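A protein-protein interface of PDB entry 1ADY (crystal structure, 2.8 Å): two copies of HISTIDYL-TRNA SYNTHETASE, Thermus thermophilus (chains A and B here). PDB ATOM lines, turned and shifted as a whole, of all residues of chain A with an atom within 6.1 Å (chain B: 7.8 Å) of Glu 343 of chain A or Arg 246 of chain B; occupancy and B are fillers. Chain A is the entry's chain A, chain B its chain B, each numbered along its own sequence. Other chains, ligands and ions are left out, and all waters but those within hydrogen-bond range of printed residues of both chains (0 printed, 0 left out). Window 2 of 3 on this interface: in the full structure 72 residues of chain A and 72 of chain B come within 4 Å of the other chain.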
ATOM      1  N   LEU A 333      10.339 -24.130 -18.307  1.00  0.00           N
ATOM      2  CA  LEU A 333      10.130 -25.237 -17.389  1.00  0.00           C
ATOM      3  C   LEU A 333       8.960 -26.110 -17.825  1.00  0.00           C
ATOM      4  O   LEU A 333       7.870 -25.612 -18.131  1.00  0.00           O
ATOM      5  CB  LEU A 333       9.906 -24.709 -15.976  1.00  0.00           C
ATOM      6  CG  LEU A 333      11.123 -24.021 -15.368  1.00  0.00           C
ATOM      7  CD1 LEU A 333      10.736 -23.310 -14.091  1.00  0.00           C
ATOM      8  CD2 LEU A 333      12.203 -25.050 -15.113  1.00  0.00           C
ATOM      9  N   GLU A 339       1.778 -31.999  -9.642  1.00  0.00           N
ATOM     10  CA  GLU A 339       2.331 -31.295  -8.490  1.00  0.00           C
ATOM     11  C   GLU A 339       3.464 -30.368  -8.931  1.00  0.00           C
ATOM     12  O   GLU A 339       3.753 -29.363  -8.273  1.00  0.00           O
ATOM     13  CB  GLU A 339       2.844 -32.305  -7.454  1.00  0.00           C
ATOM     14  CG  GLU A 339       3.295 -31.681  -6.131  1.00  0.00           C
ATOM     15  CD  GLU A 339       3.674 -32.715  -5.076  1.00  0.00           C
ATOM     16  OE1 GLU A 339       2.794 -33.505  -4.671  1.00  0.00           O
ATOM     17  OE2 GLU A 339       4.848 -32.725  -4.641  1.00  0.00           O
ATOM     18  N   ALA A 340       4.065 -30.692 -10.074  1.00  0.00           N
ATOM     19  CA  ALA A 340       5.180 -29.922 -10.627  1.00  0.00           C
ATOM     20  C   ALA A 340       4.809 -28.586 -11.267  1.00  0.00           C
ATOM     21  O   ALA A 340       5.582 -27.628 -11.183  1.00  0.00           O
ATOM     22  CB  ALA A 340       5.965 -30.773 -11.620  1.00  0.00           C
ATOM     23  N   VAL A 341       3.637 -28.512 -11.895  1.00  0.00           N
ATOM     24  CA  VAL A 341       3.209 -27.276 -12.554  1.00  0.00           C
ATOM     25  C   VAL A 341       3.301 -26.069 -11.627  1.00  0.00           C
ATOM     26  O   VAL A 341       3.936 -25.073 -11.967  1.00  0.00           O
ATOM     27  CB  VAL A 341       1.776 -27.376 -13.178  1.00  0.00           C
ATOM     28  CG1 VAL A 341       1.676 -28.590 -14.083  1.00  0.00           C
ATOM     29  CG2 VAL A 341       0.701 -27.417 -12.107  1.00  0.00           C
ATOM     30  N   ALA A 342       2.745 -26.182 -10.425  1.00  0.00           N
ATOM     31  CA  ALA A 342       2.785 -25.078  -9.476  1.00  0.00           C
ATOM     32  C   ALA A 342       4.226 -24.776  -9.082  1.00  0.00           C
ATOM     33  O   ALA A 342       4.614 -23.616  -8.950  1.00  0.00           O
ATOM     34  CB  ALA A 342       1.951 -25.404  -8.243  1.00  0.00           C
ATOM     35  N   GLU A 343       5.027 -25.825  -8.935  1.00  0.00           N
ATOM     36  CA  GLU A 343       6.422 -25.664  -8.557  1.00  0.00           C
ATOM     37  C   GLU A 343       7.217 -24.967  -9.649  1.00  0.00           C
ATOM     38  O   GLU A 343       8.127 -24.186  -9.356  1.00  0.00           O
ATOM     39  CB  GLU A 343       7.046 -27.010  -8.207  1.00  0.00           C
ATOM     40  CG  GLU A 343       6.478 -27.635  -6.933  1.00  0.00           C
ATOM     41  CD  GLU A 343       6.665 -26.765  -5.697  1.00  0.00           C
ATOM     42  OE1 GLU A 343       7.810 -26.352  -5.407  1.00  0.00           O
ATOM     43  OE2 GLU A 343       5.659 -26.500  -5.007  1.00  0.00           O
ATOM     44  N   ALA A 344       6.855 -25.230 -10.903  1.00  0.00           N
ATOM     45  CA  ALA A 344       7.521 -24.613 -12.049  1.00  0.00           C
ATOM     46  C   ALA A 344       7.276 -23.113 -11.968  1.00  0.00           C
ATOM     47  O   ALA A 344       8.196 -22.307 -12.129  1.00  0.00           O
ATOM     48  CB  ALA A 344       6.965 -25.166 -13.356  1.00  0.00           C
ATOM     49  N   PHE A 345       6.028 -22.756 -11.683  1.00  0.00           N
ATOM     50  CA  PHE A 345       5.621 -21.366 -11.551  1.00  0.00           C
ATOM     51  C   PHE A 345       6.451 -20.688 -10.466  1.00  0.00           C
ATOM     52  O   PHE A 345       7.021 -19.620 -10.688  1.00  0.00           O
ATOM     53  CB  PHE A 345       4.124 -21.305 -11.218  1.00  0.00           C
ATOM     54  CG  PHE A 345       3.642 -19.948 -10.775  1.00  0.00           C
ATOM     55  CD1 PHE A 345       3.832 -18.831 -11.574  1.00  0.00           C
ATOM     56  CD2 PHE A 345       2.986 -19.800  -9.558  1.00  0.00           C
ATOM     57  CE1 PHE A 345       3.378 -17.583 -11.167  1.00  0.00           C
ATOM     58  CE2 PHE A 345       2.524 -18.556  -9.141  1.00  0.00           C
ATOM     59  CZ  PHE A 345       2.721 -17.444  -9.947  1.00  0.00           C
ATOM     60  N   TYR A 346       6.555 -21.333  -9.310  1.00  0.00           N
ATOM     61  CA  TYR A 346       7.314 -20.788  -8.192  1.00  0.00           C
ATOM     62  C   TYR A 346       8.772 -20.569  -8.559  1.00  0.00           C
ATOM     63  O   TYR A 346       9.353 -19.531  -8.235  1.00  0.00           O
ATOM     64  CB  TYR A 346       7.219 -21.714  -6.981  1.00  0.00           C
ATOM     65  CG  TYR A 346       5.807 -21.932  -6.491  1.00  0.00           C
ATOM     66  CD1 TYR A 346       4.881 -20.892  -6.493  1.00  0.00           C
ATOM     67  CD2 TYR A 346       5.394 -23.182  -6.024  1.00  0.00           C
ATOM     68  CE1 TYR A 346       3.581 -21.090  -6.045  1.00  0.00           C
ATOM     69  CE2 TYR A 346       4.095 -23.390  -5.574  1.00  0.00           C
ATOM     70  CZ  TYR A 346       3.196 -22.340  -5.588  1.00  0.00           C
ATOM     71  OH  TYR A 346       1.914 -22.517  -5.128  1.00  0.00           O
ATOM     72  N   LEU A 347       9.356 -21.550  -9.241  1.00  0.00           N
ATOM     73  CA  LEU A 347      10.749 -21.464  -9.661  1.00  0.00           C
ATOM     74  C   LEU A 347      10.920 -20.301 -10.635  1.00  0.00           C
ATOM     75  O   LEU A 347      11.826 -19.472 -10.476  1.00  0.00           O
ATOM     76  CB  LEU A 347      11.192 -22.773 -10.317  1.00  0.00           C
ATOM     77  CG  LEU A 347      12.654 -22.880 -10.760  1.00  0.00           C
ATOM     78  CD1 LEU A 347      13.585 -22.579  -9.598  1.00  0.00           C
ATOM     79  CD2 LEU A 347      12.902 -24.272 -11.303  1.00  0.00           C
ATOM     80  N   ALA A 348      10.019 -20.223 -11.615  1.00  0.00           N
ATOM     81  CA  ALA A 348      10.042 -19.163 -12.617  1.00  0.00           C
ATOM     82  C   ALA A 348      10.042 -17.789 -11.944  1.00  0.00           C
ATOM     83  O   ALA A 348      10.895 -16.949 -12.233  1.00  0.00           O
ATOM     84  CB  ALA A 348       8.847 -19.297 -13.555  1.00  0.00           C
ATOM     85  N   LEU A 384      10.945 -30.811 -14.507  1.00  0.00           N
ATOM     86  CA  LEU A 384      10.519 -30.917 -13.118  1.00  0.00           C
ATOM     87  C   LEU A 384       9.627 -32.136 -12.934  1.00  0.00           C
ATOM     88  O   LEU A 384       8.424 -32.095 -13.199  1.00  0.00           O
ATOM     89  CB  LEU A 384       9.800 -29.652 -12.644  1.00  0.00           C
ATOM     90  CG  LEU A 384      10.710 -28.521 -12.164  1.00  0.00           C
ATOM     91  CD1 LEU A 384       9.849 -27.380 -11.659  1.00  0.00           C
ATOM     92  CD2 LEU A 384      11.635 -29.016 -11.059  1.00  0.00           C
ATOM     93  N   LEU A 389      11.823 -32.823  -7.838  1.00  0.00           N
ATOM     94  CA  LEU A 389      10.940 -32.175  -6.872  1.00  0.00           C
ATOM     95  C   LEU A 389      11.346 -32.551  -5.456  1.00  0.00           C
ATOM     96  O   LEU A 389      11.547 -31.689  -4.599  1.00  0.00           O
ATOM     97  CB  LEU A 389       9.482 -32.584  -7.096  1.00  0.00           C
ATOM     98  CG  LEU A 389       8.681 -31.815  -8.146  1.00  0.00           C
ATOM     99  CD1 LEU A 389       7.263 -32.365  -8.222  1.00  0.00           C
ATOM    100  CD2 LEU A 389       8.662 -30.339  -7.786  1.00  0.00           C
ATOM    101  N   ARG A 409      18.085 -26.016  -7.045  1.00  0.00           N
ATOM    102  CA  ARG A 409      17.359 -24.803  -7.389  1.00  0.00           C
ATOM    103  C   ARG A 409      18.194 -23.533  -7.210  1.00  0.00           C
ATOM    104  O   ARG A 409      18.101 -22.610  -8.020  1.00  0.00           O
ATOM    105  CB  ARG A 409      16.083 -24.711  -6.550  1.00  0.00           C
ATOM    106  CG  ARG A 409      14.976 -25.657  -6.973  1.00  0.00           C
ATOM    107  CD  ARG A 409      13.804 -25.532  -6.024  1.00  0.00           C
ATOM    108  NE  ARG A 409      12.516 -25.677  -6.697  1.00  0.00           N
ATOM    109  CZ  ARG A 409      11.528 -24.788  -6.613  1.00  0.00           C
ATOM    110  NH1 ARG A 409      11.680 -23.685  -5.882  1.00  0.00           N
ATOM    111  NH2 ARG A 409      10.386 -24.997  -7.263  1.00  0.00           N
ATOM    112  N   ILE B 138      -3.395 -20.336 -11.235  1.00  0.00           N
ATOM    113  CA  ILE B 138      -1.989 -19.932 -11.161  1.00  0.00           C
ATOM    114  C   ILE B 138      -1.812 -18.575 -11.858  1.00  0.00           C
ATOM    115  O   ILE B 138      -1.110 -17.687 -11.361  1.00  0.00           O
ATOM    116  CB  ILE B 138      -1.060 -20.987 -11.818  1.00  0.00           C
ATOM    117  CG1 ILE B 138      -1.023 -22.255 -10.966  1.00  0.00           C
ATOM    118  CG2 ILE B 138       0.357 -20.432 -11.989  1.00  0.00           C
ATOM    119  CD1 ILE B 138      -0.174 -23.361 -11.560  1.00  0.00           C
ATOM    120  N   VAL B 240      -5.622 -19.446  -5.378  1.00  0.00           N
ATOM    121  CA  VAL B 240      -4.915 -18.197  -5.596  1.00  0.00           C
ATOM    122  C   VAL B 240      -4.201 -17.810  -4.302  1.00  0.00           C
ATOM    123  O   VAL B 240      -2.986 -17.592  -4.302  1.00  0.00           O
ATOM    124  CB  VAL B 240      -5.881 -17.067  -6.024  1.00  0.00           C
ATOM    125  CG1 VAL B 240      -5.101 -15.791  -6.329  1.00  0.00           C
ATOM    126  CG2 VAL B 240      -6.703 -17.502  -7.231  1.00  0.00           C
ATOM    127  N   GLU B 241      -4.943 -17.793  -3.196  1.00  0.00           N
ATOM    128  CA  GLU B 241      -4.384 -17.437  -1.893  1.00  0.00           C
ATOM    129  C   GLU B 241      -3.190 -18.306  -1.543  1.00  0.00           C
ATOM    130  O   GLU B 241      -2.172 -17.809  -1.062  1.00  0.00           O
ATOM    131  CB  GLU B 241      -5.438 -17.557  -0.791  1.00  0.00           C
ATOM    132  CG  GLU B 241      -6.604 -16.596  -0.932  1.00  0.00           C
ATOM    133  CD  GLU B 241      -7.508 -16.585   0.285  1.00  0.00           C
ATOM    134  OE1 GLU B 241      -7.243 -15.790   1.212  1.00  0.00           O
ATOM    135  OE2 GLU B 241      -8.486 -17.365   0.314  1.00  0.00           O
ATOM    136  N   ARG B 242      -3.315 -19.601  -1.813  1.00  0.00           N
ATOM    137  CA  ARG B 242      -2.255 -20.557  -1.526  1.00  0.00           C
ATOM    138  C   ARG B 242      -0.980 -20.124  -2.241  1.00  0.00           C
ATOM    139  O   ARG B 242       0.083 -20.000  -1.624  1.00  0.00           O
ATOM    140  CB  ARG B 242      -2.669 -21.953  -1.991  1.00  0.00           C
ATOM    141  CG  ARG B 242      -1.920 -23.081  -1.310  1.00  0.00           C
ATOM    142  CD  ARG B 242      -2.296 -24.438  -1.900  1.00  0.00           C
ATOM    143  NE  ARG B 242      -1.262 -24.954  -2.803  1.00  0.00           N
ATOM    144  CZ  ARG B 242      -1.496 -25.478  -4.005  1.00  0.00           C
ATOM    145  NH1 ARG B 242      -2.735 -25.565  -4.482  1.00  0.00           N
ATOM    146  NH2 ARG B 242      -0.483 -25.931  -4.733  1.00  0.00           N
ATOM    147  N   HIS B 243      -1.111 -19.823  -3.529  1.00  0.00           N
ATOM    148  CA  HIS B 243       0.020 -19.397  -4.340  1.00  0.00           C
ATOM    149  C   HIS B 243       0.628 -18.092  -3.833  1.00  0.00           C
ATOM    150  O   HIS B 243       1.848 -17.995  -3.672  1.00  0.00           O
ATOM    151  CB  HIS B 243      -0.412 -19.236  -5.792  1.00  0.00           C
ATOM    152  CG  HIS B 243      -0.901 -20.503  -6.421  1.00  0.00           C
ATOM    153  ND1 HIS B 243      -0.327 -21.731  -6.170  1.00  0.00           N
ATOM    154  CD2 HIS B 243      -1.893 -20.729  -7.317  1.00  0.00           C
ATOM    155  CE1 HIS B 243      -0.935 -22.655  -6.889  1.00  0.00           C
ATOM    156  NE2 HIS B 243      -1.891 -22.076  -7.593  1.00  0.00           N
ATOM    157  N   LEU B 244      -0.224 -17.098  -3.570  1.00  0.00           N
ATOM    158  CA  LEU B 244       0.231 -15.796  -3.079  1.00  0.00           C
ATOM    159  C   LEU B 244       0.986 -15.930  -1.767  1.00  0.00           C
ATOM    160  O   LEU B 244       2.049 -15.328  -1.587  1.00  0.00           O
ATOM    161  CB  LEU B 244      -0.947 -14.836  -2.895  1.00  0.00           C
ATOM    162  CG  LEU B 244      -1.678 -14.418  -4.172  1.00  0.00           C
ATOM    163  CD1 LEU B 244      -2.792 -13.451  -3.818  1.00  0.00           C
ATOM    164  CD2 LEU B 244      -0.695 -13.787  -5.163  1.00  0.00           C
ATOM    165  N   GLU B 245       0.433 -16.725  -0.859  1.00  0.00           N
ATOM    166  CA  GLU B 245       1.043 -16.965   0.437  1.00  0.00           C
ATOM    167  C   GLU B 245       2.431 -17.586   0.248  1.00  0.00           C
ATOM    168  O   GLU B 245       3.405 -17.132   0.857  1.00  0.00           O
ATOM    169  CB  GLU B 245       0.123 -17.865   1.274  1.00  0.00           C
ATOM    170  CG  GLU B 245       0.810 -18.749   2.312  1.00  0.00           C
ATOM    171  CD  GLU B 245       0.647 -20.231   2.002  1.00  0.00           C
ATOM    172  OE1 GLU B 245      -0.490 -20.746   2.129  1.00  0.00           O
ATOM    173  OE2 GLU B 245       1.650 -20.878   1.622  1.00  0.00           O
ATOM    174  N   ARG B 246       2.525 -18.591  -0.623  1.00  0.00           N
ATOM    175  CA  ARG B 246       3.798 -19.259  -0.904  1.00  0.00           C
ATOM    176  C   ARG B 246       4.835 -18.276  -1.447  1.00  0.00           C
ATOM    177  O   ARG B 246       6.006 -18.319  -1.064  1.00  0.00           O
ATOM    178  CB  ARG B 246       3.591 -20.405  -1.901  1.00  0.00           C
ATOM    179  CG  ARG B 246       4.872 -20.917  -2.563  1.00  0.00           C
ATOM    180  CD  ARG B 246       5.885 -21.474  -1.561  1.00  0.00           C
ATOM    181  NE  ARG B 246       7.180 -21.741  -2.189  1.00  0.00           N
ATOM    182  CZ  ARG B 246       7.485 -22.857  -2.849  1.00  0.00           C
ATOM    183  NH1 ARG B 246       6.590 -23.835  -2.980  1.00  0.00           N
ATOM    184  NH2 ARG B 246       8.690 -22.996  -3.386  1.00  0.00           N
ATOM    185  N   LEU B 247       4.402 -17.400  -2.348  1.00  0.00           N
ATOM    186  CA  LEU B 247       5.290 -16.400  -2.931  1.00  0.00           C
ATOM    187  C   LEU B 247       5.522 -15.226  -1.980  1.00  0.00           C
ATOM    188  O   LEU B 247       6.194 -14.263  -2.334  1.00  0.00           O
ATOM    189  CB  LEU B 247       4.727 -15.905  -4.263  1.00  0.00           C
ATOM    190  CG  LEU B 247       4.714 -16.953  -5.378  1.00  0.00           C
ATOM    191  CD1 LEU B 247       3.828 -16.505  -6.522  1.00  0.00           C
ATOM    192  CD2 LEU B 247       6.133 -17.214  -5.852  1.00  0.00           C
ATOM    193  N   SER B 248       4.947 -15.307  -0.783  1.00  0.00           N
ATOM    194  CA  SER B 248       5.085 -14.276   0.244  1.00  0.00           C
ATOM    195  C   SER B 248       4.561 -12.888  -0.132  1.00  0.00           C
ATOM    196  O   SER B 248       5.107 -11.869   0.307  1.00  0.00           O
ATOM    197  CB  SER B 248       6.542 -14.182   0.710  1.00  0.00           C
ATOM    198  OG  SER B 248       6.964 -15.390   1.323  1.00  0.00           O
ATOM    199  N   VAL B 249       3.487 -12.849  -0.918  1.00  0.00           N
ATOM    200  CA  VAL B 249       2.883 -11.583  -1.333  1.00  0.00           C
ATOM    201  C   VAL B 249       1.884 -11.141  -0.265  1.00  0.00           C
ATOM    202  O   VAL B 249       0.820 -11.743  -0.118  1.00  0.00           O
ATOM    203  CB  VAL B 249       2.129 -11.717  -2.685  1.00  0.00           C
ATOM    204  CG1 VAL B 249       1.634 -10.350  -3.158  1.00  0.00           C
ATOM    205  CG2 VAL B 249       3.020 -12.355  -3.733  1.00  0.00           C
ATOM    206  N   TYR B 251      -1.093  -9.624   1.345  1.00  0.00           N
ATOM    207  CA  TYR B 251      -2.392  -9.155   0.879  1.00  0.00           C
ATOM    208  C   TYR B 251      -3.422  -9.171   1.999  1.00  0.00           C
ATOM    209  O   TYR B 251      -3.205  -9.768   3.051  1.00  0.00           O
ATOM    210  CB  TYR B 251      -2.889 -10.016  -0.290  1.00  0.00           C
ATOM    211  CG  TYR B 251      -3.273 -11.427   0.094  1.00  0.00           C
ATOM    212  CD1 TYR B 251      -2.312 -12.433   0.181  1.00  0.00           C
ATOM    213  CD2 TYR B 251      -4.597 -11.756   0.377  1.00  0.00           C
ATOM    214  CE1 TYR B 251      -2.662 -13.738   0.546  1.00  0.00           C
ATOM    215  CE2 TYR B 251      -4.959 -13.054   0.743  1.00  0.00           C
ATOM    216  CZ  TYR B 251      -3.989 -14.041   0.825  1.00  0.00           C
ATOM    217  OH  TYR B 251      -4.349 -15.326   1.178  1.00  0.00           O
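A ring nitrogen (ND1) of His 243 of chain B lies within hydrogen-bond range of the side-chain hydroxyl of Tyr 346 of chain A (2.6 Å). NH1 of Arg 246 of chain B lies within salt-bridge range of OE2 of Glu 343 of chain A (3.5 Å).
NH2 of Arg 409 of chain A is in salt-bridge range of OE1 of Glu 343 of chain A (3.5 Å).
Among the printed residues, merely in contact across the chains: Tyr 346 of chain A with Arg 246 of chain B, Phe 345 of chain A with Ile 138 of chain B, Phe 345 of chain A with Leu 247 of chain B, Tyr 346 of chain A with Leu 247 of chain B and Arg 409 of chain A with Arg 246 of chain B.
Glu 343 of chain A touches just one residue of chain B: Arg 246 (3.5 Å). Of chain A, only Glu 343, Tyr 346 and Arg 409 come within 4 Å of Arg 246 of chain B. No residue of chain B comes within 4 Å of Ala 344 of chain A. Of the printed residues of chain A, Ile 138 of chain B touches Phe 345 (3.5 Å). Of the printed residues of chain B, Phe 345 of chain A touches Ile 138 and Leu 247. Of the printed residues of chain B, Arg 409 of chain A touches Arg 246. Of the printed residues of chain A, His 243 of chain B touches Tyr 346. Val 240 of chain B touches none of the printed residues of chain A. The nearest printed residue of chain A that does not touch Arg 246 of chain B is Leu 347 of chain A (6.1 Å).
Hydrophobic or aromatic side chains of chain A within 4 Å of the printed part of chain B: Phe 345 and Tyr 346. Of the 12 printed residues of chain B, 4 touch a printed residue of chain A. Hydrophobic or aromatic side chains of chain B that line the printed part of chain A: Ile 138, His 243 and Leu 247. Among the printed residues, 7 pairs touch across the chains. Among the printed residues, Asp or Glu carboxylates within 4 Å of a Lys or Arg side-chain nitrogen of the other chain: Glu 343 of chain A with Arg 246 of chain B.
No position is printed for both chains.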
